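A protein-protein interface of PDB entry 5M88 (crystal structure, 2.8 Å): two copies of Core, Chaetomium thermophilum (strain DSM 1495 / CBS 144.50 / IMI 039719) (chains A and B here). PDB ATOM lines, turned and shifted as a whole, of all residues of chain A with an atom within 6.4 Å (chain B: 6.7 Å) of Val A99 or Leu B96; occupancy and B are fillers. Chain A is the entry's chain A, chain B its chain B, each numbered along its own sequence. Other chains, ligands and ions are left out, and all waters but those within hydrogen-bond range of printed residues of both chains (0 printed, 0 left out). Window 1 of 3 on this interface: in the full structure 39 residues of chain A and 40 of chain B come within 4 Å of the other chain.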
ATOM      1  N   THR A  91     -19.720  -6.751   9.248  1.00  0.00           N
ATOM      2  CA  THR A  91     -18.455  -6.832   8.520  1.00  0.00           C
ATOM      3  C   THR A  91     -18.352  -8.134   7.726  1.00  0.00           C
ATOM      4  O   THR A  91     -17.833  -8.139   6.598  1.00  0.00           O
ATOM      5  CB  THR A  91     -17.266  -6.655   9.474  1.00  0.00           C
ATOM      6  OG1 THR A  91     -16.045  -6.688   8.726  1.00  0.00           O
ATOM      7  CG2 THR A  91     -17.228  -7.736  10.537  1.00  0.00           C
ATOM      8  N   THR A  92     -18.862  -9.244   8.276  1.00  0.00           N
ATOM      9  CA  THR A  92     -18.836 -10.493   7.522  1.00  0.00           C
ATOM     10  C   THR A  92     -19.726 -10.408   6.287  1.00  0.00           C
ATOM     11  O   THR A  92     -19.344 -10.882   5.209  1.00  0.00           O
ATOM     12  CB  THR A  92     -19.248 -11.668   8.408  1.00  0.00           C
ATOM     13  OG1 THR A  92     -20.504 -11.385   9.036  1.00  0.00           O
ATOM     14  CG2 THR A  92     -18.193 -11.926   9.472  1.00  0.00           C
ATOM     15  N   GLU A  94     -20.444  -7.694   4.619  1.00  0.00           N
ATOM     16  CA  GLU A  94     -19.784  -6.813   3.658  1.00  0.00           C
ATOM     17  C   GLU A  94     -18.694  -7.560   2.895  1.00  0.00           C
ATOM     18  O   GLU A  94     -18.591  -7.452   1.662  1.00  0.00           O
ATOM     19  CB  GLU A  94     -19.205  -5.594   4.376  1.00  0.00           C
ATOM     20  CG  GLU A  94     -18.660  -4.523   3.444  1.00  0.00           C
ATOM     21  CD  GLU A  94     -18.204  -3.278   4.184  1.00  0.00           C
ATOM     22  OE1 GLU A  94     -18.244  -3.277   5.433  1.00  0.00           O
ATOM     23  OE2 GLU A  94     -17.808  -2.299   3.516  1.00  0.00           O
ATOM     24  N   GLN A  95     -17.870  -8.328   3.615  1.00  0.00           N
ATOM     25  CA  GLN A  95     -16.851  -9.132   2.945  1.00  0.00           C
ATOM     26  C   GLN A  95     -17.484 -10.139   1.988  1.00  0.00           C
ATOM     27  O   GLN A  95     -16.974 -10.362   0.880  1.00  0.00           O
ATOM     28  CB  GLN A  95     -15.976  -9.840   3.978  1.00  0.00           C
ATOM     29  CG  GLN A  95     -15.045  -8.908   4.741  1.00  0.00           C
ATOM     30  CD  GLN A  95     -14.250  -9.622   5.819  1.00  0.00           C
ATOM     31  OE1 GLN A  95     -14.537 -10.769   6.162  1.00  0.00           O
ATOM     32  NE2 GLN A  95     -13.240  -8.945   6.356  1.00  0.00           N
ATOM     33  N   LEU A  96     -18.607 -10.740   2.394  1.00  0.00           N
ATOM     34  CA  LEU A  96     -19.304 -11.689   1.531  1.00  0.00           C
ATOM     35  C   LEU A  96     -19.780 -11.019   0.248  1.00  0.00           C
ATOM     36  O   LEU A  96     -19.624 -11.568  -0.847  1.00  0.00           O
ATOM     37  CB  LEU A  96     -20.483 -12.306   2.280  1.00  0.00           C
ATOM     38  CG  LEU A  96     -21.425 -13.172   1.446  1.00  0.00           C
ATOM     39  CD1 LEU A  96     -20.673 -14.337   0.830  1.00  0.00           C
ATOM     40  CD2 LEU A  96     -22.588 -13.669   2.298  1.00  0.00           C
ATOM     41  N   ALA A  97     -20.373  -9.830   0.366  1.00  0.00           N
ATOM     42  CA  ALA A  97     -20.852  -9.128  -0.820  1.00  0.00           C
ATOM     43  C   ALA A  97     -19.703  -8.784  -1.761  1.00  0.00           C
ATOM     44  O   ALA A  97     -19.818  -8.945  -2.984  1.00  0.00           O
ATOM     45  CB  ALA A  97     -21.610  -7.865  -0.412  1.00  0.00           C
ATOM     46  N   ARG A  98     -18.575  -8.326  -1.208  1.00  0.00           N
ATOM     47  CA  ARG A  98     -17.447  -7.967  -2.064  1.00  0.00           C
ATOM     48  C   ARG A  98     -16.876  -9.192  -2.781  1.00  0.00           C
ATOM     49  O   ARG A  98     -16.588  -9.139  -3.988  1.00  0.00           O
ATOM     50  CB  ARG A  98     -16.369  -7.263  -1.241  1.00  0.00           C
ATOM     51  CG  ARG A  98     -15.221  -6.714  -2.073  1.00  0.00           C
ATOM     52  CD  ARG A  98     -14.221  -5.955  -1.214  1.00  0.00           C
ATOM     53  NE  ARG A  98     -13.657  -6.794  -0.161  1.00  0.00           N
ATOM     54  CZ  ARG A  98     -12.585  -7.565  -0.315  1.00  0.00           C
ATOM     55  NH1 ARG A  98     -11.957  -7.605  -1.483  1.00  0.00           N
ATOM     56  NH2 ARG A  98     -12.143  -8.297   0.699  1.00  0.00           N
ATOM     57  N   VAL A  99     -16.723 -10.314  -2.070  1.00  0.00           N
ATOM     58  CA  VAL A  99     -16.175 -11.496  -2.732  1.00  0.00           C
ATOM     59  C   VAL A  99     -17.176 -12.069  -3.730  1.00  0.00           C
ATOM     60  O   VAL A  99     -16.779 -12.663  -4.739  1.00  0.00           O
ATOM     61  CB  VAL A  99     -15.714 -12.556  -1.711  1.00  0.00           C
ATOM     62  CG1 VAL A  99     -14.640 -11.982  -0.791  1.00  0.00           C
ATOM     63  CG2 VAL A  99     -16.887 -13.096  -0.913  1.00  0.00           C
ATOM     64  N   ARG A 100     -18.479 -11.894  -3.490  1.00  0.00           N
ATOM     65  CA  ARG A 100     -19.466 -12.318  -4.478  1.00  0.00           C
ATOM     66  C   ARG A 100     -19.360 -11.485  -5.750  1.00  0.00           C
ATOM     67  O   ARG A 100     -19.478 -12.017  -6.863  1.00  0.00           O
ATOM     68  CB  ARG A 100     -20.874 -12.232  -3.888  1.00  0.00           C
ATOM     69  CG  ARG A 100     -21.188 -13.331  -2.886  1.00  0.00           C
ATOM     70  CD  ARG A 100     -22.612 -13.230  -2.368  1.00  0.00           C
ATOM     71  NE  ARG A 100     -23.591 -13.683  -3.351  1.00  0.00           N
ATOM     72  CZ  ARG A 100     -24.070 -14.921  -3.410  1.00  0.00           C
ATOM     73  NH1 ARG A 100     -23.663 -15.834  -2.538  1.00  0.00           N
ATOM     74  NH2 ARG A 100     -24.960 -15.246  -4.340  1.00  0.00           N
ATOM     75  N   GLU A 101     -19.140 -10.174  -5.601  1.00  0.00           N
ATOM     76  CA  GLU A 101     -18.895  -9.334  -6.773  1.00  0.00           C
ATOM     77  C   GLU A 101     -17.671  -9.816  -7.545  1.00  0.00           C
ATOM     78  O   GLU A 101     -17.698  -9.911  -8.784  1.00  0.00           O
ATOM     79  CB  GLU A 101     -18.710  -7.877  -6.346  1.00  0.00           C
ATOM     80  CG  GLU A 101     -19.933  -7.243  -5.706  1.00  0.00           C
ATOM     81  CD  GLU A 101     -19.626  -5.891  -5.084  1.00  0.00           C
ATOM     82  OE1 GLU A 101     -18.435  -5.515  -5.034  1.00  0.00           O
ATOM     83  OE2 GLU A 101     -20.575  -5.207  -4.642  1.00  0.00           O
ATOM     84  N   GLU A 102     -16.588 -10.131  -6.828  1.00  0.00           N
ATOM     85  CA  GLU A 102     -15.378 -10.603  -7.498  1.00  0.00           C
ATOM     86  C   GLU A 102     -15.619 -11.928  -8.217  1.00  0.00           C
ATOM     87  O   GLU A 102     -15.115 -12.144  -9.328  1.00  0.00           O
ATOM     88  CB  GLU A 102     -14.233 -10.731  -6.493  1.00  0.00           C
ATOM     89  CG  GLU A 102     -13.765  -9.398  -5.931  1.00  0.00           C
ATOM     90  CD  GLU A 102     -12.586  -9.536  -4.989  1.00  0.00           C
ATOM     91  OE1 GLU A 102     -12.161 -10.682  -4.729  1.00  0.00           O
ATOM     92  OE2 GLU A 102     -12.082  -8.498  -4.511  1.00  0.00           O
ATOM     93  N   LEU A 103     -16.396 -12.822  -7.601  1.00  0.00           N
ATOM     94  CA  LEU A 103     -16.715 -14.097  -8.239  1.00  0.00           C
ATOM     95  C   LEU A 103     -17.534 -13.894  -9.509  1.00  0.00           C
ATOM     96  O   LEU A 103     -17.301 -14.566 -10.521  1.00  0.00           O
ATOM     97  CB  LEU A 103     -17.461 -15.004  -7.260  1.00  0.00           C
ATOM     98  CG  LEU A 103     -17.930 -16.354  -7.809  1.00  0.00           C
ATOM     99  CD1 LEU A 103     -16.742 -17.267  -8.091  1.00  0.00           C
ATOM    100  CD2 LEU A 103     -18.911 -17.019  -6.856  1.00  0.00           C
ATOM    101  N   ALA A 104     -18.511 -12.985  -9.472  1.00  0.00           N
ATOM    102  CA  ALA A 104     -19.301 -12.711 -10.672  1.00  0.00           C
ATOM    103  C   ALA A 104     -18.428 -12.153 -11.792  1.00  0.00           C
ATOM    104  O   ALA A 104     -18.577 -12.539 -12.962  1.00  0.00           O
ATOM    105  CB  ALA A 104     -20.442 -11.746 -10.347  1.00  0.00           C
ATOM    106  N   THR B  91     -23.643 -18.703   9.605  1.00  0.00           N
ATOM    107  CA  THR B  91     -24.011 -18.965   8.219  1.00  0.00           C
ATOM    108  C   THR B  91     -23.304 -18.002   7.275  1.00  0.00           C
ATOM    109  O   THR B  91     -22.853 -18.398   6.192  1.00  0.00           O
ATOM    110  CB  THR B  91     -25.529 -18.867   8.051  1.00  0.00           C
ATOM    111  OG1 THR B  91     -26.173 -19.726   8.999  1.00  0.00           O
ATOM    112  CG2 THR B  91     -25.938 -19.287   6.647  1.00  0.00           C
ATOM    113  N   THR B  92     -23.159 -16.739   7.687  1.00  0.00           N
ATOM    114  CA  THR B  92     -22.467 -15.762   6.857  1.00  0.00           C
ATOM    115  C   THR B  92     -20.994 -16.113   6.698  1.00  0.00           C
ATOM    116  O   THR B  92     -20.446 -16.014   5.595  1.00  0.00           O
ATOM    117  CB  THR B  92     -22.626 -14.366   7.456  1.00  0.00           C
ATOM    118  OG1 THR B  92     -24.019 -14.059   7.579  1.00  0.00           O
ATOM    119  CG2 THR B  92     -21.964 -13.321   6.571  1.00  0.00           C
ATOM    120  N   ARG B  93     -20.337 -16.549   7.779  1.00  0.00           N
ATOM    121  CA  ARG B  93     -18.930 -16.926   7.667  1.00  0.00           C
ATOM    122  C   ARG B  93     -18.751 -18.162   6.790  1.00  0.00           C
ATOM    123  O   ARG B  93     -17.792 -18.244   6.009  1.00  0.00           O
ATOM    124  CB  ARG B  93     -18.333 -17.153   9.056  1.00  0.00           C
ATOM    125  CG  ARG B  93     -18.050 -15.865   9.810  1.00  0.00           C
ATOM    126  CD  ARG B  93     -17.341 -16.131  11.124  1.00  0.00           C
ATOM    127  NE  ARG B  93     -17.093 -14.902  11.874  1.00  0.00           N
ATOM    128  CZ  ARG B  93     -16.002 -14.152  11.745  1.00  0.00           C
ATOM    129  NH1 ARG B  93     -15.050 -14.503  10.889  1.00  0.00           N
ATOM    130  NH2 ARG B  93     -15.865 -13.051  12.472  1.00  0.00           N
ATOM    131  N   GLU B  94     -19.671 -19.127   6.892  1.00  0.00           N
ATOM    132  CA  GLU B  94     -19.572 -20.319   6.052  1.00  0.00           C
ATOM    133  C   GLU B  94     -19.752 -19.968   4.578  1.00  0.00           C
ATOM    134  O   GLU B  94     -18.992 -20.437   3.717  1.00  0.00           O
ATOM    135  CB  GLU B  94     -20.597 -21.365   6.491  1.00  0.00           C
ATOM    136  CG  GLU B  94     -20.435 -22.711   5.797  1.00  0.00           C
ATOM    137  CD  GLU B  94     -21.378 -23.771   6.338  1.00  0.00           C
ATOM    138  OE1 GLU B  94     -22.215 -23.441   7.205  1.00  0.00           O
ATOM    139  OE2 GLU B  94     -21.281 -24.936   5.897  1.00  0.00           O
ATOM    140  N   GLN B  95     -20.757 -19.142   4.271  1.00  0.00           N
ATOM    141  CA  GLN B  95     -20.958 -18.696   2.896  1.00  0.00           C
ATOM    142  C   GLN B  95     -19.750 -17.919   2.388  1.00  0.00           C
ATOM    143  O   GLN B  95     -19.356 -18.062   1.225  1.00  0.00           O
ATOM    144  CB  GLN B  95     -22.225 -17.847   2.803  1.00  0.00           C
ATOM    145  CG  GLN B  95     -23.510 -18.642   2.974  1.00  0.00           C
ATOM    146  CD  GLN B  95     -24.747 -17.762   2.977  1.00  0.00           C
ATOM    147  OE1 GLN B  95     -24.651 -16.538   3.074  1.00  0.00           O
ATOM    148  NE2 GLN B  95     -25.916 -18.383   2.873  1.00  0.00           N
ATOM    149  N   LEU B  96     -19.146 -17.094   3.248  1.00  0.00           N
ATOM    150  CA  LEU B  96     -17.959 -16.340   2.861  1.00  0.00           C
ATOM    151  C   LEU B  96     -16.807 -17.271   2.499  1.00  0.00           C
ATOM    152  O   LEU B  96     -16.137 -17.079   1.478  1.00  0.00           O
ATOM    153  CB  LEU B  96     -17.558 -15.398   3.996  1.00  0.00           C
ATOM    154  CG  LEU B  96     -16.223 -14.660   3.888  1.00  0.00           C
ATOM    155  CD1 LEU B  96     -16.176 -13.788   2.645  1.00  0.00           C
ATOM    156  CD2 LEU B  96     -15.975 -13.833   5.144  1.00  0.00           C
ATOM    157  N   ALA B  97     -16.562 -18.289   3.329  1.00  0.00           N
ATOM    158  CA  ALA B  97     -15.482 -19.229   3.035  1.00  0.00           C
ATOM    159  C   ALA B  97     -15.747 -19.989   1.740  1.00  0.00           C
ATOM    160  O   ALA B  97     -14.835 -20.182   0.922  1.00  0.00           O
ATOM    161  CB  ALA B  97     -15.296 -20.200   4.199  1.00  0.00           C
ATOM    162  N   ARG B  98     -16.995 -20.420   1.529  1.00  0.00           N
ATOM    163  CA  ARG B  98     -17.316 -21.164   0.314  1.00  0.00           C
ATOM    164  C   ARG B  98     -17.148 -20.296  -0.930  1.00  0.00           C
ATOM    165  O   ARG B  98     -16.603 -20.751  -1.946  1.00  0.00           O
ATOM    166  CB  ARG B  98     -18.739 -21.711   0.401  1.00  0.00           C
ATOM    167  CG  ARG B  98     -19.127 -22.616  -0.754  1.00  0.00           C
ATOM    168  CD  ARG B  98     -20.522 -23.184  -0.555  1.00  0.00           C
ATOM    169  NE  ARG B  98     -21.520 -22.126  -0.420  1.00  0.00           N
ATOM    170  CZ  ARG B  98     -22.149 -21.556  -1.443  1.00  0.00           C
ATOM    171  NH1 ARG B  98     -21.884 -21.941  -2.683  1.00  0.00           N
ATOM    172  NH2 ARG B  98     -23.042 -20.599  -1.225  1.00  0.00           N
ATOM    173  N   VAL B  99     -17.597 -19.040  -0.871  1.00  0.00           N
ATOM    174  CA  VAL B  99     -17.465 -18.166  -2.029  1.00  0.00           C
ATOM    175  C   VAL B  99     -16.004 -17.793  -2.262  1.00  0.00           C
ATOM    176  O   VAL B  99     -15.581 -17.620  -3.410  1.00  0.00           O
ATOM    177  CB  VAL B  99     -18.363 -16.926  -1.858  1.00  0.00           C
ATOM    178  CG1 VAL B  99     -18.108 -15.910  -2.958  1.00  0.00           C
ATOM    179  CG2 VAL B  99     -19.827 -17.343  -1.860  1.00  0.00           C
ATOM    180  N   ARG B 100     -15.195 -17.710  -1.202  1.00  0.00           N
ATOM    181  CA  ARG B 100     -13.767 -17.477  -1.403  1.00  0.00           C
ATOM    182  C   ARG B 100     -13.110 -18.664  -2.098  1.00  0.00           C
ATOM    183  O   ARG B 100     -12.264 -18.484  -2.986  1.00  0.00           O
ATOM    184  CB  ARG B 100     -13.075 -17.189  -0.069  1.00  0.00           C
ATOM    185  CG  ARG B 100     -13.343 -15.805   0.495  1.00  0.00           C
ATOM    186  CD  ARG B 100     -12.561 -15.590   1.782  1.00  0.00           C
ATOM    187  NE  ARG B 100     -12.883 -14.322   2.429  1.00  0.00           N
ATOM    188  CZ  ARG B 100     -12.262 -13.175   2.176  1.00  0.00           C
ATOM    189  NH1 ARG B 100     -11.282 -13.132   1.283  1.00  0.00           N
ATOM    190  NH2 ARG B 100     -12.621 -12.069   2.815  1.00  0.00           N
ATOM    191  N   GLU B 101     -13.486 -19.885  -1.705  1.00  0.00           N
ATOM    192  CA  GLU B 101     -12.995 -21.068  -2.408  1.00  0.00           C
ATOM    193  C   GLU B 101     -13.403 -21.045  -3.877  1.00  0.00           C
ATOM    194  O   GLU B 101     -12.593 -21.357  -4.761  1.00  0.00           O
ATOM    195  CB  GLU B 101     -13.506 -22.338  -1.728  1.00  0.00           C
ATOM    196  CG  GLU B 101     -13.093 -23.628  -2.425  1.00  0.00           C
ATOM    197  CD  GLU B 101     -11.595 -23.872  -2.377  1.00  0.00           C
ATOM    198  OE1 GLU B 101     -10.937 -23.371  -1.440  1.00  0.00           O
ATOM    199  OE2 GLU B 101     -11.074 -24.565  -3.278  1.00  0.00           O
ATOM    200  N   LEU B 103     -14.056 -18.433  -5.716  1.00  0.00           N
ATOM    201  CA  LEU B 103     -13.278 -17.397  -6.388  1.00  0.00           C
ATOM    202  C   LEU B 103     -11.866 -17.879  -6.698  1.00  0.00           C
ATOM    203  O   LEU B 103     -11.337 -17.619  -7.787  1.00  0.00           O
ATOM    204  CB  LEU B 103     -13.232 -16.139  -5.523  1.00  0.00           C
ATOM    205  CG  LEU B 103     -12.377 -14.986  -6.049  1.00  0.00           C
ATOM    206  CD1 LEU B 103     -13.007 -14.362  -7.290  1.00  0.00           C
ATOM    207  CD2 LEU B 103     -12.156 -13.946  -4.965  1.00  0.00           C
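The guanidinium group (NH1) of Arg A98 lies within salt-bridge range of the side-chain carboxylate (OE2) of Glu A102, 3.2 Å away.
Among the printed residues, merely in contact across the chains: Thr A92 with Thr B92, Thr A92 with Arg B93, Gln A95 with Leu B96, Leu A96 with Gln B95, Leu A96 with Leu B96, Val A99 with Leu B96, Val A99 with Val B99, Val A99 with Arg B100, Glu A102 with Leu B103 and Leu A103 with Leu B103.
Printed residues of chain B within 4 Å of Thr A92: Thr B92 (3.5 Å) and Arg B93 (3.9 Å).
Printed residues of chain B within 4 Å of Gln A95: Leu B96.
Of the printed residues of chain B, Val A99 touches Leu B96, Val B99 and Arg B100.
Printed residues of chain A within 4 Å of Thr B92: Thr A92 (3.5 Å).
Leu B96 touches three residues of chain A.
Printed residues of chain A within 4 Å of Leu B103: Glu A102 (3.3 Å) and Leu A103 (3.7 Å).
The nearest residue of chain A that does not touch Leu B96 is Thr A92 (4.5 Å).
Hydrophobic or aromatic side chains of chain B within 4 Å of the printed part of chain A: Leu B96, Val B99 and Leu B103.
Among the printed residues, no Asp or Glu carboxylate lies within 4 Å of a Lys or Arg side-chain nitrogen of the other chain.
Gln A95 touches Leu B96, and with the chains exchanged Leu A96 touches Gln B95.
Leu B96 touches its own counterpart, Leu A96.
Val B99 touches its own counterpart, Val A99.
Leu A103 touches its own counterpart, Leu B103.
11 positions are printed for both chains.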
